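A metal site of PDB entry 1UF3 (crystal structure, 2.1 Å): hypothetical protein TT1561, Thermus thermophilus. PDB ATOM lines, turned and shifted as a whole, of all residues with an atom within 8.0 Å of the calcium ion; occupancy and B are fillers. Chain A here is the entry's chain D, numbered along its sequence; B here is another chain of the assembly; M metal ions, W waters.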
ATOM      1  N   ARG A   3      -2.230  25.094 -10.286  1.00  0.00           N
ATOM      2  CA  ARG A   3      -3.482  25.768 -10.667  1.00  0.00           C
ATOM      3  C   ARG A   3      -3.522  27.124  -9.976  1.00  0.00           C
ATOM      4  O   ARG A   3      -2.570  27.505  -9.279  1.00  0.00           O
ATOM      5  CB  ARG A   3      -4.690  24.970 -10.167  1.00  0.00           C
ATOM      6  CG  ARG A   3      -4.679  23.494 -10.495  1.00  0.00           C
ATOM      7  CD  ARG A   3      -5.007  23.248 -11.939  1.00  0.00           C
ATOM      8  NE  ARG A   3      -5.023  21.815 -12.237  1.00  0.00           N
ATOM      9  CZ  ARG A   3      -5.616  21.289 -13.306  1.00  0.00           C
ATOM     10  NH1 ARG A   3      -6.242  22.082 -14.175  1.00  0.00           N
ATOM     11  NH2 ARG A   3      -5.591  19.977 -13.507  1.00  0.00           N
ATOM     12  N   THR A   4      -4.631  27.848 -10.154  1.00  0.00           N
ATOM     13  CA  THR A   4      -4.782  29.154  -9.538  1.00  0.00           C
ATOM     14  C   THR A   4      -4.908  29.011  -8.020  1.00  0.00           C
ATOM     15  O   THR A   4      -5.312  27.963  -7.507  1.00  0.00           O
ATOM     16  CB  THR A   4      -6.024  29.883 -10.052  1.00  0.00           C
ATOM     17  OG1 THR A   4      -5.914  30.049 -11.470  1.00  0.00           O
ATOM     18  CG2 THR A   4      -6.110  31.266  -9.439  1.00  0.00           C
ATOM     19  N   VAL A   5      -4.528  30.050  -7.310  1.00  0.00           N
ATOM     20  CA  VAL A   5      -4.592  30.011  -5.866  1.00  0.00           C
ATOM     21  C   VAL A   5      -5.961  30.495  -5.369  1.00  0.00           C
ATOM     22  O   VAL A   5      -6.377  31.605  -5.701  1.00  0.00           O
ATOM     23  CB  VAL A   5      -3.509  30.913  -5.252  1.00  0.00           C
ATOM     24  CG1 VAL A   5      -3.738  31.032  -3.713  1.00  0.00           C
ATOM     25  CG2 VAL A   5      -2.128  30.353  -5.578  1.00  0.00           C
ATOM     26  N   ARG A   6      -6.642  29.660  -4.589  1.00  0.00           N
ATOM     27  CA  ARG A   6      -7.931  30.052  -4.024  1.00  0.00           C
ATOM     28  C   ARG A   6      -7.902  29.878  -2.511  1.00  0.00           C
ATOM     29  O   ARG A   6      -8.444  30.717  -1.792  1.00  0.00           O
ATOM     30  CB  ARG A   6      -9.082  29.222  -4.607  1.00  0.00           C
ATOM     31  CG  ARG A   6     -10.446  29.554  -3.938  1.00  0.00           C
ATOM     32  CD  ARG A   6     -11.647  28.774  -4.539  1.00  0.00           C
ATOM     33  NE  ARG A   6     -12.882  29.062  -3.805  1.00  0.00           N
ATOM     34  CZ  ARG A   6     -13.973  28.291  -3.770  1.00  0.00           C
ATOM     35  NH1 ARG A   6     -14.021  27.142  -4.441  1.00  0.00           N
ATOM     36  NH2 ARG A   6     -14.993  28.634  -3.005  1.00  0.00           N
ATOM     37  N   TYR A   7      -7.254  28.810  -2.040  1.00  0.00           N
ATOM     38  CA  TYR A   7      -7.145  28.535  -0.608  1.00  0.00           C
ATOM     39  C   TYR A   7      -5.742  28.689  -0.065  1.00  0.00           C
ATOM     40  O   TYR A   7      -4.804  27.992  -0.481  1.00  0.00           O
ATOM     41  CB  TYR A   7      -7.652  27.139  -0.286  1.00  0.00           C
ATOM     42  CG  TYR A   7      -9.100  26.952  -0.677  1.00  0.00           C
ATOM     43  CD1 TYR A   7      -9.438  26.567  -1.979  1.00  0.00           C
ATOM     44  CD2 TYR A   7     -10.122  27.248   0.219  1.00  0.00           C
ATOM     45  CE1 TYR A   7     -10.757  26.492  -2.366  1.00  0.00           C
ATOM     46  CE2 TYR A   7     -11.461  27.180  -0.158  1.00  0.00           C
ATOM     47  CZ  TYR A   7     -11.765  26.802  -1.461  1.00  0.00           C
ATOM     48  OH  TYR A   7     -13.070  26.754  -1.880  1.00  0.00           O
ATOM     49  N   ALA A  28      -1.246  20.949   4.864  1.00  0.00           N
ATOM     50  CA  ALA A  28      -1.464  21.368   3.505  1.00  0.00           C
ATOM     51  C   ALA A  28      -2.114  20.335   2.586  1.00  0.00           C
ATOM     52  O   ALA A  28      -3.112  20.620   1.960  1.00  0.00           O
ATOM     53  CB  ALA A  28      -0.151  21.837   2.896  1.00  0.00           C
ATOM     54  N   PRO A  29      -1.559  19.118   2.513  1.00  0.00           N
ATOM     55  CA  PRO A  29      -2.152  18.100   1.631  1.00  0.00           C
ATOM     56  C   PRO A  29      -3.586  17.713   2.004  1.00  0.00           C
ATOM     57  O   PRO A  29      -4.436  17.532   1.129  1.00  0.00           O
ATOM     58  CB  PRO A  29      -1.185  16.916   1.772  1.00  0.00           C
ATOM     59  CG  PRO A  29       0.125  17.585   2.101  1.00  0.00           C
ATOM     60  CD  PRO A  29      -0.304  18.624   3.102  1.00  0.00           C
ATOM     61  N   THR A  31      -5.813  19.531   3.444  1.00  0.00           N
ATOM     62  CA  THR A  31      -6.743  20.628   3.193  1.00  0.00           C
ATOM     63  C   THR A  31      -6.909  21.016   1.722  1.00  0.00           C
ATOM     64  O   THR A  31      -7.920  21.617   1.362  1.00  0.00           O
ATOM     65  CB  THR A  31      -6.310  21.886   3.917  1.00  0.00           C
ATOM     66  OG1 THR A  31      -5.050  22.315   3.410  1.00  0.00           O
ATOM     67  CG2 THR A  31      -6.205  21.633   5.428  1.00  0.00           C
ATOM     68  N   GLY A  32      -5.919  20.701   0.897  1.00  0.00           N
ATOM     69  CA  GLY A  32      -5.983  21.089  -0.507  1.00  0.00           C
ATOM     70  C   GLY A  32      -5.462  22.509  -0.670  1.00  0.00           C
ATOM     71  O   GLY A  32      -5.602  23.094  -1.745  1.00  0.00           O
ATOM     72  N   ALA A  33      -4.848  23.070   0.368  1.00  0.00           N
ATOM     73  CA  ALA A  33      -4.332  24.441   0.266  1.00  0.00           C
ATOM     74  C   ALA A  33      -3.444  24.594  -0.962  1.00  0.00           C
ATOM     75  O   ALA A  33      -2.610  23.724  -1.251  1.00  0.00           O
ATOM     76  CB  ALA A  33      -3.542  24.805   1.531  1.00  0.00           C
ATOM     77  N   ASP A  34      -3.620  25.710  -1.663  1.00  0.00           N
ATOM     78  CA  ASP A  34      -2.877  26.028  -2.878  1.00  0.00           C
ATOM     79  C   ASP A  34      -1.645  26.873  -2.589  1.00  0.00           C
ATOM     80  O   ASP A  34      -0.756  27.033  -3.437  1.00  0.00           O
ATOM     81  CB  ASP A  34      -3.769  26.787  -3.856  1.00  0.00           C
ATOM     82  CG  ASP A  34      -5.123  26.114  -4.043  1.00  0.00           C
ATOM     83  OD1 ASP A  34      -5.147  24.927  -4.454  1.00  0.00           O
ATOM     84  OD2 ASP A  34      -6.165  26.768  -3.762  1.00  0.00           O
ATOM     85  N   ALA A  35      -1.570  27.422  -1.390  1.00  0.00           N
ATOM     86  CA  ALA A  35      -0.442  28.249  -1.037  1.00  0.00           C
ATOM     87  C   ALA A  35      -0.338  28.427   0.468  1.00  0.00           C
ATOM     88  O   ALA A  35      -1.262  28.097   1.210  1.00  0.00           O
ATOM     89  CB  ALA A  35      -0.572  29.590  -1.723  1.00  0.00           C
ATOM     90  N   LEU A  64       4.775  24.016  -2.156  1.00  0.00           N
ATOM     91  CA  LEU A  64       3.658  24.916  -2.436  1.00  0.00           C
ATOM     92  C   LEU A  64       4.121  26.360  -2.467  1.00  0.00           C
ATOM     93  O   LEU A  64       5.079  26.734  -1.780  1.00  0.00           O
ATOM     94  CB  LEU A  64       2.588  24.812  -1.332  1.00  0.00           C
ATOM     95  CG  LEU A  64       1.585  23.652  -1.264  1.00  0.00           C
ATOM     96  CD1 LEU A  64       0.630  23.880  -0.080  1.00  0.00           C
ATOM     97  CD2 LEU A  64       0.798  23.555  -2.563  1.00  0.00           C
ATOM     98  N   MET B   1      -8.051  24.593  -4.945  1.00  0.00           N
ATOM     99  CA  MET B   1      -9.345  23.964  -4.554  1.00  0.00           C
ATOM    100  C   MET B   1      -9.198  23.020  -3.354  1.00  0.00           C
ATOM    101  O   MET B   1      -8.106  22.459  -3.138  1.00  0.00           O
ATOM    102  CB  MET B   1      -9.932  23.182  -5.730  1.00  0.00           C
ATOM    103  CG  MET B   1     -10.308  24.030  -6.930  1.00  0.00           C
ATOM    104  SD  MET B   1     -11.554  25.487  -6.513  1.00  0.00           S
ATOM    105  CE  MET B   1     -13.186  24.422  -6.272  1.00  0.00           C
ATOM    106  N   ARG B   2     -10.274  22.862  -2.589  1.00  0.00           N
ATOM    107  CA  ARG B   2     -10.268  21.961  -1.434  1.00  0.00           C
ATOM    108  C   ARG B   2     -10.026  20.576  -2.022  1.00  0.00           C
ATOM    109  O   ARG B   2     -10.399  20.322  -3.165  1.00  0.00           O
ATOM    110  CB  ARG B   2     -11.629  21.960  -0.740  1.00  0.00           C
ATOM    111  CG  ARG B   2     -11.979  23.221   0.025  1.00  0.00           C
ATOM    112  CD  ARG B   2     -13.372  23.064   0.642  1.00  0.00           C
ATOM    113  NE  ARG B   2     -13.674  24.088   1.639  1.00  0.00           N
ATOM    114  CZ  ARG B   2     -14.186  25.285   1.360  1.00  0.00           C
ATOM    115  NH1 ARG B   2     -14.479  25.629   0.105  1.00  0.00           N
ATOM    116  NH2 ARG B   2     -14.391  26.139   2.356  1.00  0.00           N
ATOM    117  N   ARG B   3      -9.420  19.669  -1.261  1.00  0.00           N
ATOM    118  CA  ARG B   3      -9.162  18.355  -1.831  1.00  0.00           C
ATOM    119  C   ARG B   3     -10.416  17.513  -1.949  1.00  0.00           C
ATOM    120  O   ARG B   3     -10.510  16.630  -2.802  1.00  0.00           O
ATOM    121  CB  ARG B   3      -8.094  17.605  -1.041  1.00  0.00           C
ATOM    122  CG  ARG B   3      -8.387  17.356   0.396  1.00  0.00           C
ATOM    123  CD  ARG B   3      -7.418  16.292   0.915  1.00  0.00           C
ATOM    124  NE  ARG B   3      -7.885  14.935   0.654  1.00  0.00           N
ATOM    125  CZ  ARG B   3      -8.553  14.194   1.533  1.00  0.00           C
ATOM    126  NH1 ARG B   3      -8.826  14.683   2.737  1.00  0.00           N
ATOM    127  NH2 ARG B   3      -8.964  12.977   1.208  1.00  0.00           N
ATOM    128  N   ARG B 105     -13.624  16.598  -7.154  1.00  0.00           N
ATOM    129  CA  ARG B 105     -12.597  16.361  -6.149  1.00  0.00           C
ATOM    130  C   ARG B 105     -13.192  15.588  -4.983  1.00  0.00           C
ATOM    131  O   ARG B 105     -14.272  15.892  -4.485  1.00  0.00           O
ATOM    132  CB  ARG B 105     -11.975  17.684  -5.684  1.00  0.00           C
ATOM    133  CG  ARG B 105     -11.268  18.413  -6.844  1.00  0.00           C
ATOM    134  CD  ARG B 105     -10.357  19.541  -6.367  1.00  0.00           C
ATOM    135  NE  ARG B 105      -9.600  20.165  -7.467  1.00  0.00           N
ATOM    136  CZ  ARG B 105     -10.072  21.105  -8.284  1.00  0.00           C
ATOM    137  NH1 ARG B 105     -11.307  21.561  -8.163  1.00  0.00           N
ATOM    138  NH2 ARG B 105      -9.290  21.597  -9.244  1.00  0.00           N
HETATM  139 CA    CA M   1      -5.957  23.025  -4.102  1.00  0.00          CA
HETATM  140  O   HOH W   1      -6.019  20.558  -4.511  1.00  0.00           O
HETATM  141  O   HOH W   2      -5.731  23.108  -6.684  1.00  0.00           O
HETATM  142  O   HOH W   3      -3.424  22.412  -4.272  1.00  0.00           O
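The guanidinium group of Arg 6 lies close to the side-chain sulfur of Met 1 of chain B, 3.6 Å away.
OD2 of Asp 34 sits at hydrogen-bond distance from N of Arg 6 (3.0 Å).
O of Tyr 7 sits at hydrogen-bond distance from N of Asp 34 (2.8 Å).
Of the 17 residues printed, 3 come within 4 Å of the calcium ion.
The calcium ion is bound by OD1 of Asp 34 (2.1 Å), O of Gly 32 (2.4 Å), O of Met 1 of chain B (2.4 Å), water W1 (2.5 Å), water W2 (2.6 Å), water W3 (2.6 Å) and N of Met 1 of chain B (2.7 Å).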
